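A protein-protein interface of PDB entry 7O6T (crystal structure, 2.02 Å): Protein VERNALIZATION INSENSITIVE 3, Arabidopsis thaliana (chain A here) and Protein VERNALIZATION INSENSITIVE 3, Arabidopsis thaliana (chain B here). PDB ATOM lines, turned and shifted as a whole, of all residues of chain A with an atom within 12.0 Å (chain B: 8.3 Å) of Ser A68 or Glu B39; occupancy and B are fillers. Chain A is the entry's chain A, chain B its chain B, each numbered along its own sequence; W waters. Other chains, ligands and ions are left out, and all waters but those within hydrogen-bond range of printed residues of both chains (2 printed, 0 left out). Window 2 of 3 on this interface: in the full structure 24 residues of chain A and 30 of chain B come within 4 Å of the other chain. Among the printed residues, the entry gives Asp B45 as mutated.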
ATOM      1  N   LEU A  57      -3.554   0.605 -17.600  1.00  0.00           N
ATOM      2  CA  LEU A  57      -4.277  -0.571 -17.133  1.00  0.00           C
ATOM      3  C   LEU A  57      -5.320  -1.011 -18.163  1.00  0.00           C
ATOM      4  O   LEU A  57      -5.376  -2.181 -18.538  1.00  0.00           O
ATOM      5  CB  LEU A  57      -4.933  -0.302 -15.769  1.00  0.00           C
ATOM      6  CG  LEU A  57      -5.729  -1.476 -15.167  1.00  0.00           C
ATOM      7  CD1 LEU A  57      -4.862  -2.725 -15.031  1.00  0.00           C
ATOM      8  CD2 LEU A  57      -6.335  -1.054 -13.828  1.00  0.00           C
ATOM      9  N   GLN A  59      -5.247  -0.482 -21.397  1.00  0.00           N
ATOM     10  CA  GLN A  59      -4.512  -1.093 -22.514  1.00  0.00           C
ATOM     11  C   GLN A  59      -4.083  -2.530 -22.201  1.00  0.00           C
ATOM     12  O   GLN A  59      -4.274  -3.434 -23.023  1.00  0.00           O
ATOM     13  CB  GLN A  59      -3.279  -0.282 -22.886  1.00  0.00           C
ATOM     14  CG  GLN A  59      -3.588   0.966 -23.684  1.00  0.00           C
ATOM     15  CD  GLN A  59      -2.340   1.719 -24.114  1.00  0.00           C
ATOM     16  OE1 GLN A  59      -1.331   1.133 -24.539  1.00  0.00           O
ATOM     17  NE2 GLN A  59      -2.411   3.026 -24.026  1.00  0.00           N
ATOM     18  N   GLN A  60      -3.516  -2.724 -21.003  1.00  0.00           N
ATOM     19  CA  GLN A  60      -3.073  -4.026 -20.560  1.00  0.00           C
ATOM     20  C   GLN A  60      -4.227  -5.036 -20.544  1.00  0.00           C
ATOM     21  O   GLN A  60      -4.065  -6.184 -20.989  1.00  0.00           O
ATOM     22  CB  GLN A  60      -2.404  -3.974 -19.184  1.00  0.00           C
ATOM     23  CG  GLN A  60      -1.122  -3.167 -19.123  1.00  0.00           C
ATOM     24  CD  GLN A  60      -0.667  -2.857 -17.688  1.00  0.00           C
ATOM     25  OE1 GLN A  60      -1.439  -2.391 -16.806  1.00  0.00           O
ATOM     26  NE2 GLN A  60       0.611  -3.091 -17.451  1.00  0.00           N
ATOM     27  N   LEU A  61      -5.388  -4.613 -20.036  1.00  0.00           N
ATOM     28  CA  LEU A  61      -6.524  -5.524 -19.910  1.00  0.00           C
ATOM     29  C   LEU A  61      -7.077  -5.867 -21.282  1.00  0.00           C
ATOM     30  O   LEU A  61      -7.422  -7.035 -21.528  1.00  0.00           O
ATOM     31  CB  LEU A  61      -7.605  -4.959 -18.998  1.00  0.00           C
ATOM     32  CG  LEU A  61      -7.173  -4.833 -17.516  1.00  0.00           C
ATOM     33  CD1 LEU A  61      -8.368  -4.446 -16.689  1.00  0.00           C
ATOM     34  CD2 LEU A  61      -6.535  -6.111 -16.963  1.00  0.00           C
ATOM     35  N   VAL A  62      -7.155  -4.850 -22.159  1.00  0.00           N
ATOM     36  CA  VAL A  62      -7.620  -5.018 -23.528  1.00  0.00           C
ATOM     37  C   VAL A  62      -6.656  -5.963 -24.257  1.00  0.00           C
ATOM     38  O   VAL A  62      -7.101  -6.886 -24.939  1.00  0.00           O
ATOM     39  CB  VAL A  62      -7.768  -3.685 -24.280  1.00  0.00           C
ATOM     40  CG1 VAL A  62      -7.986  -3.906 -25.782  1.00  0.00           C
ATOM     41  CG2 VAL A  62      -8.924  -2.853 -23.699  1.00  0.00           C
ATOM     42  N   ASP A  63      -5.343  -5.770 -24.071  1.00  0.00           N
ATOM     43  CA  ASP A  63      -4.360  -6.619 -24.737  1.00  0.00           C
ATOM     44  C   ASP A  63      -4.381  -8.050 -24.233  1.00  0.00           C
ATOM     45  O   ASP A  63      -4.238  -8.995 -25.007  1.00  0.00           O
ATOM     46  CB  ASP A  63      -2.966  -6.010 -24.653  1.00  0.00           C
ATOM     47  CG  ASP A  63      -2.814  -4.789 -25.583  1.00  0.00           C
ATOM     48  OD1 ASP A  63      -3.781  -4.410 -26.293  1.00  0.00           O
ATOM     49  OD2 ASP A  63      -1.744  -4.187 -25.584  1.00  0.00           O
ATOM     50  N   THR A  64      -4.520  -8.226 -22.919  1.00  0.00           N
ATOM     51  CA  THR A  64      -4.656  -9.569 -22.324  1.00  0.00           C
ATOM     52  C   THR A  64      -5.893 -10.327 -22.873  1.00  0.00           C
ATOM     53  O   THR A  64      -5.849 -11.506 -23.194  1.00  0.00           O
ATOM     54  CB  THR A  64      -4.765  -9.464 -20.800  1.00  0.00           C
ATOM     55  OG1 THR A  64      -3.624  -8.765 -20.305  1.00  0.00           O
ATOM     56  CG2 THR A  64      -4.863 -10.803 -20.154  1.00  0.00           C
ATOM     57  N   PHE A  65      -7.022  -9.631 -22.928  1.00  0.00           N
ATOM     58  CA  PHE A  65      -8.246 -10.174 -23.484  1.00  0.00           C
ATOM     59  C   PHE A  65      -8.086 -10.577 -24.968  1.00  0.00           C
ATOM     60  O   PHE A  65      -8.528 -11.655 -25.387  1.00  0.00           O
ATOM     61  CB  PHE A  65      -9.370  -9.147 -23.331  1.00  0.00           C
ATOM     62  CG  PHE A  65     -10.692  -9.618 -23.862  1.00  0.00           C
ATOM     63  CD1 PHE A  65     -11.483 -10.475 -23.115  1.00  0.00           C
ATOM     64  CD2 PHE A  65     -11.147  -9.201 -25.117  1.00  0.00           C
ATOM     65  CE1 PHE A  65     -12.716 -10.910 -23.595  1.00  0.00           C
ATOM     66  CE2 PHE A  65     -12.376  -9.612 -25.598  1.00  0.00           C
ATOM     67  CZ  PHE A  65     -13.171 -10.473 -24.829  1.00  0.00           C
ATOM     68  N   SER A  66      -7.425  -9.718 -25.745  1.00  0.00           N
ATOM     69  CA  SER A  66      -7.169  -9.937 -27.167  1.00  0.00           C
ATOM     70  C   SER A  66      -6.295 -11.159 -27.396  1.00  0.00           C
ATOM     71  O   SER A  66      -6.543 -11.975 -28.304  1.00  0.00           O
ATOM     72  CB  SER A  66      -6.490  -8.714 -27.799  1.00  0.00           C
ATOM     73  OG  SER A  66      -7.352  -7.602 -27.752  1.00  0.00           O
ATOM     74  N   GLU A  67      -5.269 -11.284 -26.564  1.00  0.00           N
ATOM     75  CA  GLU A  67      -4.344 -12.392 -26.651  1.00  0.00           C
ATOM     76  C   GLU A  67      -5.074 -13.696 -26.371  1.00  0.00           C
ATOM     77  O   GLU A  67      -4.852 -14.687 -27.033  1.00  0.00           O
ATOM     78  CB  GLU A  67      -3.176 -12.199 -25.685  1.00  0.00           C
ATOM     79  CG  GLU A  67      -2.111 -13.275 -25.929  1.00  0.00           C
ATOM     80  CD  GLU A  67      -0.797 -13.024 -25.190  1.00  0.00           C
ATOM     81  OE1 GLU A  67      -0.451 -11.855 -24.896  1.00  0.00           O
ATOM     82  OE2 GLU A  67      -0.125 -14.021 -24.898  1.00  0.00           O
ATOM     83  N   SER A  68      -5.953 -13.673 -25.359  1.00  0.00           N
ATOM     84  CA  SER A  68      -6.754 -14.843 -25.007  1.00  0.00           C
ATOM     85  C   SER A  68      -7.607 -15.335 -26.180  1.00  0.00           C
ATOM     86  O   SER A  68      -7.677 -16.520 -26.436  1.00  0.00           O
ATOM     87  CB  SER A  68      -7.640 -14.567 -23.811  1.00  0.00           C
ATOM     88  OG  SER A  68      -8.207 -15.788 -23.375  1.00  0.00           O
ATOM     89  N   ILE A  69      -8.220 -14.405 -26.917  1.00  0.00           N
ATOM     90  CA  ILE A  69      -8.959 -14.730 -28.141  1.00  0.00           C
ATOM     91  C   ILE A  69      -8.111 -15.439 -29.203  1.00  0.00           C
ATOM     92  O   ILE A  69      -8.530 -16.469 -29.749  1.00  0.00           O
ATOM     93  CB  ILE A  69      -9.639 -13.485 -28.756  1.00  0.00           C
ATOM     94  CG1 ILE A  69     -10.704 -12.935 -27.794  1.00  0.00           C
ATOM     95  CG2 ILE A  69     -10.255 -13.837 -30.108  1.00  0.00           C
ATOM     96  CD1 ILE A  69     -11.289 -11.585 -28.199  1.00  0.00           C
ATOM     97  N   LEU A  70      -6.918 -14.902 -29.493  1.00  0.00           N
ATOM     98  CA  LEU A  70      -6.014 -15.485 -30.471  1.00  0.00           C
ATOM     99  C   LEU A  70      -5.576 -16.888 -30.091  1.00  0.00           C
ATOM    100  O   LEU A  70      -5.425 -17.731 -30.959  1.00  0.00           O
ATOM    101  CB  LEU A  70      -4.756 -14.636 -30.626  1.00  0.00           C
ATOM    102  CG  LEU A  70      -4.950 -13.209 -31.117  1.00  0.00           C
ATOM    103  CD1 LEU A  70      -3.611 -12.500 -31.130  1.00  0.00           C
ATOM    104  CD2 LEU A  70      -5.579 -13.215 -32.489  1.00  0.00           C
ATOM    105  N   SER A  71      -5.393 -17.132 -28.788  1.00  0.00           N
ATOM    106  CA  SER A  71      -4.892 -18.420 -28.313  1.00  0.00           C
ATOM    107  C   SER A  71      -5.924 -19.583 -28.457  1.00  0.00           C
ATOM    108  O   SER A  71      -5.556 -20.755 -28.316  1.00  0.00           O
ATOM    109  CB  SER A  71      -4.413 -18.302 -26.866  1.00  0.00           C
ATOM    110  OG  SER A  71      -5.513 -18.222 -25.999  1.00  0.00           O
ATOM    111  N   LYS A  72      -7.193 -19.245 -28.744  1.00  0.00           N
ATOM    112  CA  LYS A  72      -8.249 -20.233 -29.036  1.00  0.00           C
ATOM    113  C   LYS A  72      -7.932 -21.084 -30.276  1.00  0.00           C
ATOM    114  O   LYS A  72      -8.280 -22.265 -30.334  1.00  0.00           O
ATOM    115  CB  LYS A  72      -9.607 -19.549 -29.245  1.00  0.00           C
ATOM    116  CG  LYS A  72     -10.110 -18.696 -28.087  1.00  0.00           C
ATOM    117  CD  LYS A  72     -10.460 -19.506 -26.846  1.00  0.00           C
ATOM    118  CE  LYS A  72      -9.247 -19.816 -25.980  1.00  0.00           C
ATOM    119  NZ  LYS A  72      -9.547 -19.630 -24.537  1.00  0.00           N
ATOM    120  N   LYS A  73      -7.277 -20.464 -31.268  1.00  0.00           N
ATOM    121  CA  LYS A  73      -6.858 -21.132 -32.497  1.00  0.00           C
ATOM    122  C   LYS A  73      -6.068 -22.393 -32.123  1.00  0.00           C
ATOM    123  O   LYS A  73      -5.181 -22.365 -31.253  1.00  0.00           O
ATOM    124  CB  LYS A  73      -6.048 -20.167 -33.381  1.00  0.00           C
ATOM    125  CG  LYS A  73      -5.502 -20.750 -34.671  1.00  0.00           C
ATOM    126  CD  LYS A  73      -6.560 -21.068 -35.720  1.00  0.00           C
ATOM    127  CE  LYS A  73      -5.950 -21.947 -36.809  1.00  0.00           C
ATOM    128  NZ  LYS A  73      -6.542 -21.685 -38.138  1.00  0.00           N
ATOM    129  OXT LYS A  73      -6.346 -23.474 -32.661  1.00  0.00           O
ATOM    130  N   PHE B  27     -15.437  -8.738 -21.252  1.00  0.00           N
ATOM    131  CA  PHE B  27     -14.271  -8.996 -20.415  1.00  0.00           C
ATOM    132  C   PHE B  27     -14.716  -9.695 -19.152  1.00  0.00           C
ATOM    133  O   PHE B  27     -14.091 -10.660 -18.745  1.00  0.00           O
ATOM    134  CB  PHE B  27     -13.549  -7.696 -20.035  1.00  0.00           C
ATOM    135  CG  PHE B  27     -12.324  -7.907 -19.210  1.00  0.00           C
ATOM    136  CD1 PHE B  27     -12.388  -7.985 -17.839  1.00  0.00           C
ATOM    137  CD2 PHE B  27     -11.068  -8.019 -19.831  1.00  0.00           C
ATOM    138  CE1 PHE B  27     -11.244  -8.160 -17.087  1.00  0.00           C
ATOM    139  CE2 PHE B  27      -9.921  -8.194 -19.073  1.00  0.00           C
ATOM    140  CZ  PHE B  27     -10.006  -8.261 -17.710  1.00  0.00           C
ATOM    141  N   TRP B  30     -15.884 -13.255 -19.809  1.00  0.00           N
ATOM    142  CA  TRP B  30     -14.681 -14.048 -20.058  1.00  0.00           C
ATOM    143  C   TRP B  30     -13.932 -14.356 -18.770  1.00  0.00           C
ATOM    144  O   TRP B  30     -13.604 -15.516 -18.480  1.00  0.00           O
ATOM    145  CB  TRP B  30     -13.777 -13.326 -21.051  1.00  0.00           C
ATOM    146  CG  TRP B  30     -12.398 -13.859 -21.167  1.00  0.00           C
ATOM    147  CD1 TRP B  30     -11.982 -14.920 -21.939  1.00  0.00           C
ATOM    148  CD2 TRP B  30     -11.221 -13.330 -20.542  1.00  0.00           C
ATOM    149  NE1 TRP B  30     -10.605 -15.073 -21.835  1.00  0.00           N
ATOM    150  CE2 TRP B  30     -10.123 -14.116 -20.973  1.00  0.00           C
ATOM    151  CE3 TRP B  30     -10.985 -12.259 -19.671  1.00  0.00           C
ATOM    152  CZ2 TRP B  30      -8.831 -13.879 -20.533  1.00  0.00           C
ATOM    153  CZ3 TRP B  30      -9.710 -12.030 -19.227  1.00  0.00           C
ATOM    154  CH2 TRP B  30      -8.638 -12.835 -19.665  1.00  0.00           C
ATOM    155  N   TYR B  31     -13.708 -13.320 -17.965  1.00  0.00           N
ATOM    156  CA  TYR B  31     -12.961 -13.414 -16.684  1.00  0.00           C
ATOM    157  C   TYR B  31     -13.613 -14.446 -15.765  1.00  0.00           C
ATOM    158  O   TYR B  31     -12.896 -15.285 -15.202  1.00  0.00           O
ATOM    159  CB  TYR B  31     -12.879 -12.053 -15.983  1.00  0.00           C
ATOM    160  CG  TYR B  31     -12.092 -12.113 -14.704  1.00  0.00           C
ATOM    161  CD1 TYR B  31     -10.704 -12.167 -14.713  1.00  0.00           C
ATOM    162  CD2 TYR B  31     -12.741 -12.275 -13.490  1.00  0.00           C
ATOM    163  CE1 TYR B  31      -9.979 -12.276 -13.536  1.00  0.00           C
ATOM    164  CE2 TYR B  31     -12.031 -12.407 -12.308  1.00  0.00           C
ATOM    165  CZ  TYR B  31     -10.644 -12.407 -12.329  1.00  0.00           C
ATOM    166  OH  TYR B  31      -9.964 -12.549 -11.156  1.00  0.00           O
ATOM    167  N   ARG B  34     -14.495 -18.165 -18.672  1.00  0.00           N
ATOM    168  CA  ARG B  34     -13.650 -18.761 -19.752  1.00  0.00           C
ATOM    169  C   ARG B  34     -12.151 -18.488 -19.566  1.00  0.00           C
ATOM    170  O   ARG B  34     -11.358 -19.212 -20.181  1.00  0.00           O
ATOM    171  CB  ARG B  34     -14.136 -18.290 -21.128  1.00  0.00           C
ATOM    172  CG  ARG B  34     -15.315 -19.116 -21.630  1.00  0.00           C
ATOM    173  CD  ARG B  34     -15.896 -18.635 -22.935  1.00  0.00           C
ATOM    174  NE  ARG B  34     -16.746 -17.488 -22.699  1.00  0.00           N
ATOM    175  CZ  ARG B  34     -16.452 -16.226 -22.994  1.00  0.00           C
ATOM    176  NH1 ARG B  34     -15.301 -15.918 -23.572  1.00  0.00           N
ATOM    177  NH2 ARG B  34     -17.329 -15.273 -22.722  1.00  0.00           N
ATOM    178  N   ALA B  35     -11.753 -17.497 -18.768  1.00  0.00           N
ATOM    179  CA  ALA B  35     -10.335 -17.242 -18.535  1.00  0.00           C
ATOM    180  C   ALA B  35      -9.718 -18.435 -17.817  1.00  0.00           C
ATOM    181  O   ALA B  35     -10.290 -18.944 -16.844  1.00  0.00           O
ATOM    182  CB  ALA B  35     -10.137 -15.961 -17.743  1.00  0.00           C
ATOM    183  N   THR B  36      -8.544 -18.864 -18.293  1.00  0.00           N
ATOM    184  CA  THR B  36      -7.800 -19.960 -17.682  1.00  0.00           C
ATOM    185  C   THR B  36      -7.185 -19.459 -16.378  1.00  0.00           C
ATOM    186  O   THR B  36      -7.193 -18.236 -16.117  1.00  0.00           O
ATOM    187  CB  THR B  36      -6.658 -20.427 -18.599  1.00  0.00           C
ATOM    188  OG1 THR B  36      -5.749 -19.340 -18.793  1.00  0.00           O
ATOM    189  CG2 THR B  36      -7.187 -20.857 -19.938  1.00  0.00           C
ATOM    190  N   HIS B  37      -6.628 -20.382 -15.581  1.00  0.00           N
ATOM    191  CA  HIS B  37      -6.018 -20.022 -14.298  1.00  0.00           C
ATOM    192  C   HIS B  37      -4.861 -19.038 -14.493  1.00  0.00           C
ATOM    193  O   HIS B  37      -4.682 -18.114 -13.701  1.00  0.00           O
ATOM    194  CB  HIS B  37      -5.556 -21.262 -13.518  1.00  0.00           C
ATOM    195  CG  HIS B  37      -6.675 -22.007 -12.855  1.00  0.00           C
ATOM    196  ND1 HIS B  37      -7.265 -21.578 -11.685  1.00  0.00           N
ATOM    197  CD2 HIS B  37      -7.318 -23.148 -13.205  1.00  0.00           C
ATOM    198  CE1 HIS B  37      -8.222 -22.423 -11.341  1.00  0.00           C
ATOM    199  NE2 HIS B  37      -8.272 -23.387 -12.243  1.00  0.00           N
ATOM    200  N   ARG B  38      -4.089 -19.251 -15.560  1.00  0.00           N
ATOM    201  CA  ARG B  38      -2.961 -18.378 -15.983  1.00  0.00           C
ATOM    202  C   ARG B  38      -3.493 -16.984 -16.361  1.00  0.00           C
ATOM    203  O   ARG B  38      -2.902 -15.991 -15.930  1.00  0.00           O
ATOM    204  CB  ARG B  38      -2.234 -19.046 -17.152  1.00  0.00           C
ATOM    205  CG  ARG B  38      -1.149 -18.219 -17.825  1.00  0.00           C
ATOM    206  CD  ARG B  38      -1.090 -18.537 -19.312  1.00  0.00           C
ATOM    207  NE  ARG B  38      -1.164 -17.303 -20.072  1.00  0.00           N
ATOM    208  CZ  ARG B  38      -0.164 -16.430 -20.205  1.00  0.00           C
ATOM    209  NH1 ARG B  38       1.021 -16.670 -19.660  1.00  0.00           N
ATOM    210  NH2 ARG B  38      -0.351 -15.317 -20.898  1.00  0.00           N
ATOM    211  N   GLU B  39      -4.546 -16.914 -17.175  1.00  0.00           N
ATOM    212  CA  GLU B  39      -5.085 -15.636 -17.622  1.00  0.00           C
ATOM    213  C   GLU B  39      -5.653 -14.836 -16.446  1.00  0.00           C
ATOM    214  O   GLU B  39      -5.487 -13.624 -16.390  1.00  0.00           O
ATOM    215  CB  GLU B  39      -6.106 -15.859 -18.711  1.00  0.00           C
ATOM    216  CG  GLU B  39      -5.477 -16.369 -20.003  1.00  0.00           C
ATOM    217  CD  GLU B  39      -6.486 -16.917 -20.993  1.00  0.00           C
ATOM    218  OE1 GLU B  39      -7.605 -17.315 -20.573  1.00  0.00           O
ATOM    219  OE2 GLU B  39      -6.170 -16.914 -22.209  1.00  0.00           O
ATOM    220  N   VAL B  40      -6.293 -15.536 -15.501  1.00  0.00           N
ATOM    221  CA  VAL B  40      -6.826 -14.940 -14.281  1.00  0.00           C
ATOM    222  C   VAL B  40      -5.705 -14.360 -13.466  1.00  0.00           C
ATOM    223  O   VAL B  40      -5.818 -13.259 -12.937  1.00  0.00           O
ATOM    224  CB  VAL B  40      -7.622 -15.976 -13.442  1.00  0.00           C
ATOM    225  CG1 VAL B  40      -7.846 -15.500 -12.010  1.00  0.00           C
ATOM    226  CG2 VAL B  40      -8.955 -16.280 -14.121  1.00  0.00           C
ATOM    227  N   ARG B  41      -4.615 -15.120 -13.349  1.00  0.00           N
ATOM    228  CA  ARG B  41      -3.393 -14.696 -12.621  1.00  0.00           C
ATOM    229  C   ARG B  41      -2.878 -13.411 -13.285  1.00  0.00           C
ATOM    230  O   ARG B  41      -2.580 -12.474 -12.544  1.00  0.00           O
ATOM    231  CB  ARG B  41      -2.374 -15.841 -12.617  1.00  0.00           C
ATOM    232  CG  ARG B  41      -1.080 -15.565 -11.864  1.00  0.00           C
ATOM    233  CD  ARG B  41      -1.235 -15.590 -10.345  1.00  0.00           C
ATOM    234  NE  ARG B  41      -1.752 -14.340  -9.792  1.00  0.00           N
ATOM    235  CZ  ARG B  41      -2.373 -14.210  -8.620  1.00  0.00           C
ATOM    236  NH1 ARG B  41      -2.584 -15.265  -7.852  1.00  0.00           N
ATOM    237  NH2 ARG B  41      -2.789 -13.017  -8.226  1.00  0.00           N
ATOM    238  N   VAL B  42      -2.804 -13.375 -14.621  1.00  0.00           N
ATOM    239  CA  VAL B  42      -2.325 -12.198 -15.341  1.00  0.00           C
ATOM    240  C   VAL B  42      -3.176 -10.959 -15.029  1.00  0.00           C
ATOM    241  O   VAL B  42      -2.651  -9.871 -14.726  1.00  0.00           O
ATOM    242  CB  VAL B  42      -2.252 -12.465 -16.850  1.00  0.00           C
ATOM    243  CG1 VAL B  42      -2.047 -11.181 -17.634  1.00  0.00           C
ATOM    244  CG2 VAL B  42      -1.097 -13.443 -17.148  1.00  0.00           C
ATOM    245  N   VAL B  43      -4.501 -11.134 -15.094  1.00  0.00           N
ATOM    246  CA  VAL B  43      -5.430 -10.047 -14.842  1.00  0.00           C
ATOM    247  C   VAL B  43      -5.296  -9.566 -13.404  1.00  0.00           C
ATOM    248  O   VAL B  43      -5.174  -8.362 -13.157  1.00  0.00           O
ATOM    249  CB  VAL B  43      -6.882 -10.461 -15.161  1.00  0.00           C
ATOM    250  CG1 VAL B  43      -7.881  -9.452 -14.601  1.00  0.00           C
ATOM    251  CG2 VAL B  43      -7.054 -10.599 -16.658  1.00  0.00           C
ATOM    252  N   LYS B  44      -5.321 -10.506 -12.457  1.00  0.00           N
ATOM    253  CA  LYS B  44      -5.221 -10.199 -11.050  1.00  0.00           C
ATOM    254  C   LYS B  44      -3.929  -9.450 -10.687  1.00  0.00           C
ATOM    255  O   LYS B  44      -3.974  -8.524  -9.918  1.00  0.00           O
ATOM    256  CB  LYS B  44      -5.324 -11.477 -10.224  1.00  0.00           C
ATOM    257  CG  LYS B  44      -6.741 -11.997 -10.042  1.00  0.00           C
ATOM    258  CD  LYS B  44      -6.744 -13.249  -9.161  1.00  0.00           C
ATOM    259  CE  LYS B  44      -8.140 -13.544  -8.606  1.00  0.00           C
ATOM    260  NZ  LYS B  44      -8.155 -14.736  -7.725  1.00  0.00           N
ATOM    261  N   ASP B  45      -2.790  -9.863 -11.252  1.00  0.00           N
ATOM    262  CA  ASP B  45      -1.518  -9.165 -11.034  1.00  0.00           C
ATOM    263  C   ASP B  45      -1.544  -7.716 -11.545  1.00  0.00           C
ATOM    264  O   ASP B  45      -1.098  -6.808 -10.847  1.00  0.00           O
ATOM    265  CB  ASP B  45      -0.345  -9.932 -11.656  1.00  0.00           C
ATOM    266  CG  ASP B  45      -0.100 -11.275 -10.987  1.00  0.00           C
ATOM    267  OD1 ASP B  45      -0.694 -11.541  -9.904  1.00  0.00           O
ATOM    268  OD2 ASP B  45       0.691 -12.080 -11.557  1.00  0.00           O
ATOM    269  N   PHE B  46      -2.081  -7.497 -12.753  1.00  0.00           N
ATOM    270  CA  PHE B  46      -2.217  -6.139 -13.287  1.00  0.00           C
ATOM    271  C   PHE B  46      -3.068  -5.245 -12.353  1.00  0.00           C
ATOM    272  O   PHE B  46      -2.695  -4.120 -12.025  1.00  0.00           O
ATOM    273  CB  PHE B  46      -2.829  -6.137 -14.683  1.00  0.00           C
ATOM    274  CG  PHE B  46      -1.877  -6.500 -15.784  1.00  0.00           C
ATOM    275  CD1 PHE B  46      -0.606  -5.927 -15.856  1.00  0.00           C
ATOM    276  CD2 PHE B  46      -2.281  -7.350 -16.820  1.00  0.00           C
ATOM    277  CE1 PHE B  46       0.243  -6.231 -16.913  1.00  0.00           C
ATOM    278  CE2 PHE B  46      -1.436  -7.661 -17.856  1.00  0.00           C
ATOM    279  CZ  PHE B  46      -0.164  -7.099 -17.912  1.00  0.00           C
HETATM  280  O   HOH W   1      -1.106  -2.528 -13.523  1.00  0.00           O
HETATM  281  O   HOH W   2      -9.612 -18.426 -22.040  1.00  0.00           O
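O of Gln A60 sits at hydrogen-bond distance from OG1 of Thr A64, at 2.7 Å. OG of Ser A71 lies within hydrogen-bond range of O of Ser A68 (2.8 Å). O of Trp B30 lies within hydrogen-bond range of N of Ala B35. The backbone NH (N) of Thr B36 lies within hydrogen-bond range of the side-chain carboxylate (OE1) of Glu B39 (2.9 Å).
OG of Ser A68 sits at hydrogen-bond distance from NE1 of Trp B30. The side-chain hydroxyl of Ser A68 sits at hydrogen-bond distance from the side-chain carboxylate of Glu B39 (2.6 Å).
Of the printed residues of chain B, Gln A60 touches Phe B46. Of the printed residues of chain B, Thr A64 touches Val B42 and Phe B46. Ser A68 touches just these residues of chain B: Trp B30 (2.9 Å) and Glu B39 (2.6 Å). Ile A69 touches none of the printed residues of chain B. No residue of chain A comes within 4 Å of Ala B35. Glu B39 touches one residue of chain A. No residue of chain A comes within 4 Å of Val B40. Of the printed residues of chain A, Phe B46 touches Leu A57, Gln A60 and Thr A64. The nearest residue of chain B that does not touch Ser A68 is Ala B35 (5.5 Å). The nearest printed residue of chain B that does not touch Gln A60 is Val B42 (6.3 Å).
Leu A57 touches Phe B46. Gln A60 touches Phe B46 (NE2 to CE1, 3.2 Å). Phe B27 touches Leu A61 (CE2 to O, 3.7 Å). CG1 of Val B42 touches CG2 of Thr A64, at 3.8 Å. Phe B46 touches Thr A64 (CE2 to OG1, 3.5 Å). CE1 of Phe A65 touches CB of Trp B30, at 3.7 Å.
Water W2 lies within hydrogen-bond range of O of Arg B34 (2.7 Å), OE1 of Glu B39 (2.7 Å), NZ of Lys A72 (2.8 Å) and OG of Ser A68 (3.3 Å). Water W1 lies within hydrogen-bond range of O of Phe B46 (2.7 Å) and OE1 of Gln A60 (3.3 Å).
Of the 16 printed residues of chain B, 5 touch a printed residue of chain A. Hydrophobic or aromatic side chains of chain B that line the printed part of chain A: Phe B27, Trp B30, Val B42 and Phe B46. Along chain A the printed residues that touch a printed residue of chain B span positions 57 to 68.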
